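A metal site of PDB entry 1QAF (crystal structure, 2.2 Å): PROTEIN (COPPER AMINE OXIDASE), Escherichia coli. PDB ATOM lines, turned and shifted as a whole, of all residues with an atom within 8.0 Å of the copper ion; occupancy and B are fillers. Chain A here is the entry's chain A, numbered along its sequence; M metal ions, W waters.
A ring nitrogen (ND1) of His 519 is in hydrogen-bond range of the backbone carbonyl oxygen of Thr 517, at 2.8 Å.
A ring nitrogen (NE2) of His 684 is in hydrogen-bond range of the side-chain carboxylate (OE1) of Glu 690, at 2.7 Å.
N of Thr 682 sits at hydrogen-bond distance from O of His 521, 2.9 Å away.
ND1 of His 521 lies within hydrogen-bond range of OH of Tyr 463 (3.4 Å).
Within 4 Å of the copper ion: His 519, His 521 and His 684.
The nearest printed residue that does not touch the copper ion is TPQ 461 (4.7 Å).
The copper ion is bound by a ring nitrogen (NE2) of His 521 (2.2 Å), a ring nitrogen (ND1) of His 684 (2.2 Å), a ring nitrogen (NE2) of His 519 (2.3 Å) and water W1 (2.6 Å).
The copper ion has four donor atoms within binding distance.
Slightly farther from the copper ion lies water W2 (2.7 Å).
Water W2 lies within hydrogen-bond range of O2 of TPQ 461 (2.8 Å) and the side-chain sulfur of Met 694 (3.4 Å).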
ATOM      1  N   VAL A 362      10.479  10.867  14.970  1.00  0.00           N
ATOM      2  CA  VAL A 362      10.433  10.295  16.286  1.00  0.00           C
ATOM      3  C   VAL A 362      11.340   9.063  16.262  1.00  0.00           C
ATOM      4  O   VAL A 362      10.993   7.896  16.018  1.00  0.00           O
ATOM      5  CB  VAL A 362       9.000   9.926  16.654  1.00  0.00           C
ATOM      6  CG1 VAL A 362       8.839   9.563  18.113  1.00  0.00           C
ATOM      7  CG2 VAL A 362       8.112  11.091  16.224  1.00  0.00           C
ATOM      8  N   TYR A 364      13.908   6.340  18.048  1.00  0.00           N
ATOM      9  CA  TYR A 364      14.051   5.633  19.317  1.00  0.00           C
ATOM     10  C   TYR A 364      15.482   5.318  19.723  1.00  0.00           C
ATOM     11  O   TYR A 364      16.375   5.397  18.869  1.00  0.00           O
ATOM     12  CB  TYR A 364      13.187   4.365  19.256  1.00  0.00           C
ATOM     13  CG  TYR A 364      11.728   4.707  19.533  1.00  0.00           C
ATOM     14  CD1 TYR A 364      10.953   5.280  18.537  1.00  0.00           C
ATOM     15  CD2 TYR A 364      11.181   4.515  20.798  1.00  0.00           C
ATOM     16  CE1 TYR A 364       9.646   5.648  18.798  1.00  0.00           C
ATOM     17  CE2 TYR A 364       9.872   4.853  21.072  1.00  0.00           C
ATOM     18  CZ  TYR A 364       9.126   5.420  20.061  1.00  0.00           C
ATOM     19  OH  TYR A 364       7.815   5.749  20.368  1.00  0.00           O
ATOM     20  N   ASN A 460      -0.061   5.450  17.346  1.00  0.00           N
ATOM     21  CA  ASN A 460      -0.297   5.697  18.767  1.00  0.00           C
ATOM     22  C   ASN A 460      -0.105   7.102  19.242  1.00  0.00           C
ATOM     23  O   ASN A 460      -0.598   7.446  20.286  1.00  0.00           O
ATOM     24  CB  ASN A 460       0.715   4.843  19.542  1.00  0.00           C
ATOM     25  CG  ASN A 460       2.158   5.123  19.191  1.00  0.00           C
ATOM     26  OD1 ASN A 460       2.965   5.546  20.029  1.00  0.00           O
ATOM     27  ND2 ASN A 460       2.413   4.862  17.918  1.00  0.00           N
ATOM     28  N   TPQ A 461       0.609   7.907  18.494  1.00  0.00           N
ATOM     29  CA  TPQ A 461       0.879   9.278  18.933  1.00  0.00           C
ATOM     30  CB  TPQ A 461       2.093  10.004  18.309  1.00  0.00           C
ATOM     31  C   TPQ A 461      -0.012  10.355  18.401  1.00  0.00           C
ATOM     32  O   TPQ A 461      -0.494  10.298  17.221  1.00  0.00           O
ATOM     33  C1  TPQ A 461       3.266   8.961  18.341  1.00  0.00           C
ATOM     34  C2  TPQ A 461       4.074   8.797  19.493  1.00  0.00           C
ATOM     35  O2  TPQ A 461       3.840   9.427  20.544  1.00  0.00           O
ATOM     36  C3  TPQ A 461       5.186   7.865  19.536  1.00  0.00           C
ATOM     37  C4  TPQ A 461       5.409   7.130  18.367  1.00  0.00           C
ATOM     38  O4  TPQ A 461       6.416   6.214  18.400  1.00  0.00           O
ATOM     39  C5  TPQ A 461       4.635   7.286  17.238  1.00  0.00           C
ATOM     40  O5  TPQ A 461       4.989   6.557  16.259  1.00  0.00           O
ATOM     41  C6  TPQ A 461       3.562   8.239  17.257  1.00  0.00           C
ATOM     42  N   TYR A 463      -0.465  14.569  17.993  1.00  0.00           N
ATOM     43  CA  TYR A 463       0.253  15.793  17.885  1.00  0.00           C
ATOM     44  C   TYR A 463      -0.689  16.938  17.631  1.00  0.00           C
ATOM     45  O   TYR A 463      -1.589  16.839  16.774  1.00  0.00           O
ATOM     46  CB  TYR A 463       1.202  15.666  16.686  1.00  0.00           C
ATOM     47  CG  TYR A 463       2.227  14.559  16.888  1.00  0.00           C
ATOM     48  CD1 TYR A 463       3.154  14.590  17.955  1.00  0.00           C
ATOM     49  CD2 TYR A 463       2.293  13.482  16.005  1.00  0.00           C
ATOM     50  CE1 TYR A 463       4.020  13.528  18.112  1.00  0.00           C
ATOM     51  CE2 TYR A 463       3.198  12.456  16.132  1.00  0.00           C
ATOM     52  CZ  TYR A 463       4.074  12.488  17.208  1.00  0.00           C
ATOM     53  OH  TYR A 463       4.994  11.478  17.338  1.00  0.00           O
ATOM     54  N   ALA A 481       2.271  17.022  22.376  1.00  0.00           N
ATOM     55  CA  ALA A 481       2.350  15.595  22.106  1.00  0.00           C
ATOM     56  C   ALA A 481       1.594  14.861  23.216  1.00  0.00           C
ATOM     57  O   ALA A 481       1.827  15.116  24.398  1.00  0.00           O
ATOM     58  CB  ALA A 481       3.826  15.156  22.158  1.00  0.00           C
ATOM     59  N   THR A 482       0.700  13.973  22.830  1.00  0.00           N
ATOM     60  CA  THR A 482      -0.121  13.160  23.693  1.00  0.00           C
ATOM     61  C   THR A 482      -0.339  11.823  23.010  1.00  0.00           C
ATOM     62  O   THR A 482       0.313  11.476  22.005  1.00  0.00           O
ATOM     63  CB  THR A 482      -1.397  13.846  24.204  1.00  0.00           C
ATOM     64  OG1 THR A 482      -2.107  12.921  25.048  1.00  0.00           O
ATOM     65  CG2 THR A 482      -2.444  14.241  23.149  1.00  0.00           C
ATOM     66  N   ILE A 484      -0.639   7.453  23.226  1.00  0.00           N
ATOM     67  CA  ILE A 484      -0.252   6.254  23.923  1.00  0.00           C
ATOM     68  C   ILE A 484       1.205   5.920  23.679  1.00  0.00           C
ATOM     69  O   ILE A 484       1.525   5.885  22.501  1.00  0.00           O
ATOM     70  CB  ILE A 484      -1.059   5.048  23.324  1.00  0.00           C
ATOM     71  CG1 ILE A 484      -2.586   5.247  23.365  1.00  0.00           C
ATOM     72  CG2 ILE A 484      -0.705   3.826  24.210  1.00  0.00           C
ATOM     73  CD1 ILE A 484      -3.225   5.921  24.575  1.00  0.00           C
ATOM     74  N   GLU A 485       1.981   5.685  24.727  1.00  0.00           N
ATOM     75  CA  GLU A 485       3.367   5.347  24.368  1.00  0.00           C
ATOM     76  C   GLU A 485       3.640   3.982  23.747  1.00  0.00           C
ATOM     77  O   GLU A 485       2.899   3.037  24.040  1.00  0.00           O
ATOM     78  CB  GLU A 485       4.185   5.312  25.672  1.00  0.00           C
ATOM     79  CG  GLU A 485       4.969   6.618  25.785  1.00  0.00           C
ATOM     80  CD  GLU A 485       5.429   6.879  27.205  1.00  0.00           C
ATOM     81  OE1 GLU A 485       6.496   6.286  27.482  1.00  0.00           O
ATOM     82  OE2 GLU A 485       4.698   7.647  27.891  1.00  0.00           O
ATOM     83  N   ALA A 486       4.666   3.868  22.924  1.00  0.00           N
ATOM     84  CA  ALA A 486       5.147   2.672  22.243  1.00  0.00           C
ATOM     85  C   ALA A 486       5.908   1.948  23.371  1.00  0.00           C
ATOM     86  O   ALA A 486       6.956   2.467  23.798  1.00  0.00           O
ATOM     87  CB  ALA A 486       6.225   3.103  21.233  1.00  0.00           C
ATOM     88  N   THR A 517      10.208   2.898  26.128  1.00  0.00           N
ATOM     89  CA  THR A 517      11.503   3.132  25.513  1.00  0.00           C
ATOM     90  C   THR A 517      11.761   4.585  25.174  1.00  0.00           C
ATOM     91  O   THR A 517      10.977   5.227  24.476  1.00  0.00           O
ATOM     92  CB  THR A 517      11.663   2.267  24.266  1.00  0.00           C
ATOM     93  OG1 THR A 517      11.325   0.909  24.559  1.00  0.00           O
ATOM     94  CG2 THR A 517      12.944   2.432  23.483  1.00  0.00           C
ATOM     95  N   THR A 518      12.887   5.074  25.702  1.00  0.00           N
ATOM     96  CA  THR A 518      13.300   6.444  25.452  1.00  0.00           C
ATOM     97  C   THR A 518      13.340   6.760  23.968  1.00  0.00           C
ATOM     98  O   THR A 518      13.737   5.944  23.156  1.00  0.00           O
ATOM     99  CB  THR A 518      14.726   6.665  26.015  1.00  0.00           C
ATOM    100  OG1 THR A 518      14.556   6.579  27.446  1.00  0.00           O
ATOM    101  CG2 THR A 518      15.213   8.076  25.740  1.00  0.00           C
ATOM    102  N   HIS A 519      12.898   7.960  23.584  1.00  0.00           N
ATOM    103  CA  HIS A 519      12.936   8.355  22.181  1.00  0.00           C
ATOM    104  C   HIS A 519      12.915   9.889  22.165  1.00  0.00           C
ATOM    105  O   HIS A 519      12.837  10.511  23.209  1.00  0.00           O
ATOM    106  CB  HIS A 519      11.708   7.897  21.366  1.00  0.00           C
ATOM    107  CG  HIS A 519      10.467   8.237  22.138  1.00  0.00           C
ATOM    108  ND1 HIS A 519       9.997   7.557  23.255  1.00  0.00           N
ATOM    109  CD2 HIS A 519       9.650   9.297  21.877  1.00  0.00           C
ATOM    110  CE1 HIS A 519       8.878   8.119  23.674  1.00  0.00           C
ATOM    111  NE2 HIS A 519       8.669   9.090  22.824  1.00  0.00           N
ATOM    112  N   GLN A 520      12.946  10.523  21.006  1.00  0.00           N
ATOM    113  CA  GLN A 520      12.876  11.965  20.932  1.00  0.00           C
ATOM    114  C   GLN A 520      11.688  12.290  20.042  1.00  0.00           C
ATOM    115  O   GLN A 520      11.152  11.461  19.304  1.00  0.00           O
ATOM    116  CB  GLN A 520      14.145  12.401  20.170  1.00  0.00           C
ATOM    117  CG  GLN A 520      15.347  12.400  21.128  1.00  0.00           C
ATOM    118  CD  GLN A 520      16.525  13.065  20.476  1.00  0.00           C
ATOM    119  OE1 GLN A 520      16.680  14.163  21.013  1.00  0.00           O
ATOM    120  NE2 GLN A 520      17.203  12.473  19.487  1.00  0.00           N
ATOM    121  N   HIS A 521      11.238  13.524  20.031  1.00  0.00           N
ATOM    122  CA  HIS A 521      10.145  14.042  19.211  1.00  0.00           C
ATOM    123  C   HIS A 521      10.865  15.263  18.609  1.00  0.00           C
ATOM    124  O   HIS A 521      11.180  16.143  19.424  1.00  0.00           O
ATOM    125  CB  HIS A 521       8.857  14.437  19.853  1.00  0.00           C
ATOM    126  CG  HIS A 521       8.071  13.330  20.453  1.00  0.00           C
ATOM    127  ND1 HIS A 521       7.297  12.503  19.641  1.00  0.00           N
ATOM    128  CD2 HIS A 521       7.968  12.896  21.724  1.00  0.00           C
ATOM    129  CE1 HIS A 521       6.737  11.520  20.317  1.00  0.00           C
ATOM    130  NE2 HIS A 521       7.119  11.815  21.533  1.00  0.00           N
ATOM    131  N   TYR A 523      10.475  18.365  15.992  1.00  0.00           N
ATOM    132  CA  TYR A 523       9.684  18.972  14.945  1.00  0.00           C
ATOM    133  C   TYR A 523      10.467  20.019  14.134  1.00  0.00           C
ATOM    134  O   TYR A 523      11.368  20.632  14.708  1.00  0.00           O
ATOM    135  CB  TYR A 523       8.554  19.754  15.672  1.00  0.00           C
ATOM    136  CG  TYR A 523       7.842  18.932  16.710  1.00  0.00           C
ATOM    137  CD1 TYR A 523       6.712  18.202  16.333  1.00  0.00           C
ATOM    138  CD2 TYR A 523       8.205  18.910  18.035  1.00  0.00           C
ATOM    139  CE1 TYR A 523       6.018  17.434  17.233  1.00  0.00           C
ATOM    140  CE2 TYR A 523       7.531  18.133  18.957  1.00  0.00           C
ATOM    141  CZ  TYR A 523       6.445  17.399  18.540  1.00  0.00           C
ATOM    142  OH  TYR A 523       5.772  16.640  19.464  1.00  0.00           O
ATOM    143  N   HIS A 608       8.851  18.872  28.664  1.00  0.00           N
ATOM    144  CA  HIS A 608       9.576  17.624  28.689  1.00  0.00           C
ATOM    145  C   HIS A 608      11.027  18.060  28.526  1.00  0.00           C
ATOM    146  O   HIS A 608      11.322  19.173  28.083  1.00  0.00           O
ATOM    147  CB  HIS A 608       9.242  16.721  27.508  1.00  0.00           C
ATOM    148  CG  HIS A 608       8.431  15.488  27.733  1.00  0.00           C
ATOM    149  ND1 HIS A 608       7.846  14.764  26.697  1.00  0.00           N
ATOM    150  CD2 HIS A 608       8.102  14.901  28.917  1.00  0.00           C
ATOM    151  CE1 HIS A 608       7.198  13.741  27.277  1.00  0.00           C
ATOM    152  NE2 HIS A 608       7.308  13.783  28.607  1.00  0.00           N
ATOM    153  N   THR A 682      12.031  17.305  21.908  1.00  0.00           N
ATOM    154  CA  THR A 682      12.063  16.770  23.236  1.00  0.00           C
ATOM    155  C   THR A 682      12.788  15.444  23.339  1.00  0.00           C
ATOM    156  O   THR A 682      12.810  14.732  22.345  1.00  0.00           O
ATOM    157  CB  THR A 682      10.618  16.547  23.769  1.00  0.00           C
ATOM    158  OG1 THR A 682       9.894  15.512  23.060  1.00  0.00           O
ATOM    159  CG2 THR A 682       9.802  17.835  23.730  1.00  0.00           C
ATOM    160  N   THR A 683      13.342  15.168  24.517  1.00  0.00           N
ATOM    161  CA  THR A 683      14.021  13.903  24.721  1.00  0.00           C
ATOM    162  C   THR A 683      13.009  13.283  25.693  1.00  0.00           C
ATOM    163  O   THR A 683      12.860  13.797  26.784  1.00  0.00           O
ATOM    164  CB  THR A 683      15.411  13.977  25.326  1.00  0.00           C
ATOM    165  OG1 THR A 683      16.229  14.270  24.199  1.00  0.00           O
ATOM    166  CG2 THR A 683      15.736  12.566  25.768  1.00  0.00           C
ATOM    167  N   HIS A 684      12.327  12.214  25.317  1.00  0.00           N
ATOM    168  CA  HIS A 684      11.350  11.668  26.224  1.00  0.00           C
ATOM    169  C   HIS A 684      11.702  10.437  27.023  1.00  0.00           C
ATOM    170  O   HIS A 684      11.759   9.332  26.498  1.00  0.00           O
ATOM    171  CB  HIS A 684      10.088  11.474  25.329  1.00  0.00           C
ATOM    172  CG  HIS A 684       8.901  11.026  26.129  1.00  0.00           C
ATOM    173  ND1 HIS A 684       7.732  10.560  25.618  1.00  0.00           N
ATOM    174  CD2 HIS A 684       8.678  10.893  27.462  1.00  0.00           C
ATOM    175  CE1 HIS A 684       6.821  10.207  26.498  1.00  0.00           C
ATOM    176  NE2 HIS A 684       7.400  10.391  27.651  1.00  0.00           N
ATOM    177  N   VAL A 685      11.957  10.655  28.293  1.00  0.00           N
ATOM    178  CA  VAL A 685      12.269   9.606  29.258  1.00  0.00           C
ATOM    179  C   VAL A 685      10.905   9.529  29.950  1.00  0.00           C
ATOM    180  O   VAL A 685      10.453  10.533  30.508  1.00  0.00           O
ATOM    181  CB  VAL A 685      13.374   9.939  30.271  1.00  0.00           C
ATOM    182  CG1 VAL A 685      13.646   8.824  31.280  1.00  0.00           C
ATOM    183  CG2 VAL A 685      14.595  10.374  29.476  1.00  0.00           C
ATOM    184  N   ALA A 686      10.236   8.393  29.901  1.00  0.00           N
ATOM    185  CA  ALA A 686       8.936   8.140  30.461  1.00  0.00           C
ATOM    186  C   ALA A 686       8.809   7.988  31.959  1.00  0.00           C
ATOM    187  O   ALA A 686       9.748   7.844  32.730  1.00  0.00           O
ATOM    188  CB  ALA A 686       8.247   6.955  29.798  1.00  0.00           C
ATOM    189  N   GLU A 690       2.490   8.777  32.681  1.00  0.00           N
ATOM    190  CA  GLU A 690       2.125   8.808  31.271  1.00  0.00           C
ATOM    191  C   GLU A 690       1.524   7.521  30.727  1.00  0.00           C
ATOM    192  O   GLU A 690       1.476   7.370  29.481  1.00  0.00           O
ATOM    193  CB  GLU A 690       3.370   9.207  30.421  1.00  0.00           C
ATOM    194  CG  GLU A 690       4.147  10.345  31.011  1.00  0.00           C
ATOM    195  CD  GLU A 690       5.534  10.620  30.426  1.00  0.00           C
ATOM    196  OE1 GLU A 690       6.267   9.709  29.961  1.00  0.00           O
ATOM    197  OE2 GLU A 690       5.960  11.820  30.428  1.00  0.00           O
ATOM    198  N   MET A 694      -0.827   9.450  27.960  1.00  0.00           N
ATOM    199  CA  MET A 694       0.056  10.561  28.193  1.00  0.00           C
ATOM    200  C   MET A 694      -0.498  11.961  28.236  1.00  0.00           C
ATOM    201  O   MET A 694      -1.101  12.482  27.292  1.00  0.00           O
ATOM    202  CB  MET A 694       1.151  10.714  27.105  1.00  0.00           C
ATOM    203  CG  MET A 694       1.892   9.465  26.653  1.00  0.00           C
ATOM    204  SD  MET A 694       3.058   9.725  25.279  1.00  0.00           S
ATOM    205  CE  MET A 694       2.076   9.056  23.923  1.00  0.00           C
ATOM    206  N   GLU A 697       2.339  17.241  26.515  1.00  0.00           N
ATOM    207  CA  GLU A 697       3.581  17.947  26.803  1.00  0.00           C
ATOM    208  C   GLU A 697       3.747  18.926  25.625  1.00  0.00           C
ATOM    209  O   GLU A 697       3.522  18.678  24.423  1.00  0.00           O
ATOM    210  CB  GLU A 697       4.756  16.969  26.825  1.00  0.00           C
ATOM    211  CG  GLU A 697       4.502  15.900  27.878  1.00  0.00           C
ATOM    212  CD  GLU A 697       4.817  16.423  29.272  1.00  0.00           C
ATOM    213  OE1 GLU A 697       5.142  17.618  29.538  1.00  0.00           O
ATOM    214  OE2 GLU A 697       4.667  15.587  30.165  1.00  0.00           O
HETATM  215 CU    CU M   1       7.237  10.745  23.441  1.00  0.00          CU
HETATM  216  O   HOH W   1       5.349  12.505  23.709  1.00  0.00           O
HETATM  217  O   HOH W   2       5.343   8.926  22.860  1.00  0.00           O
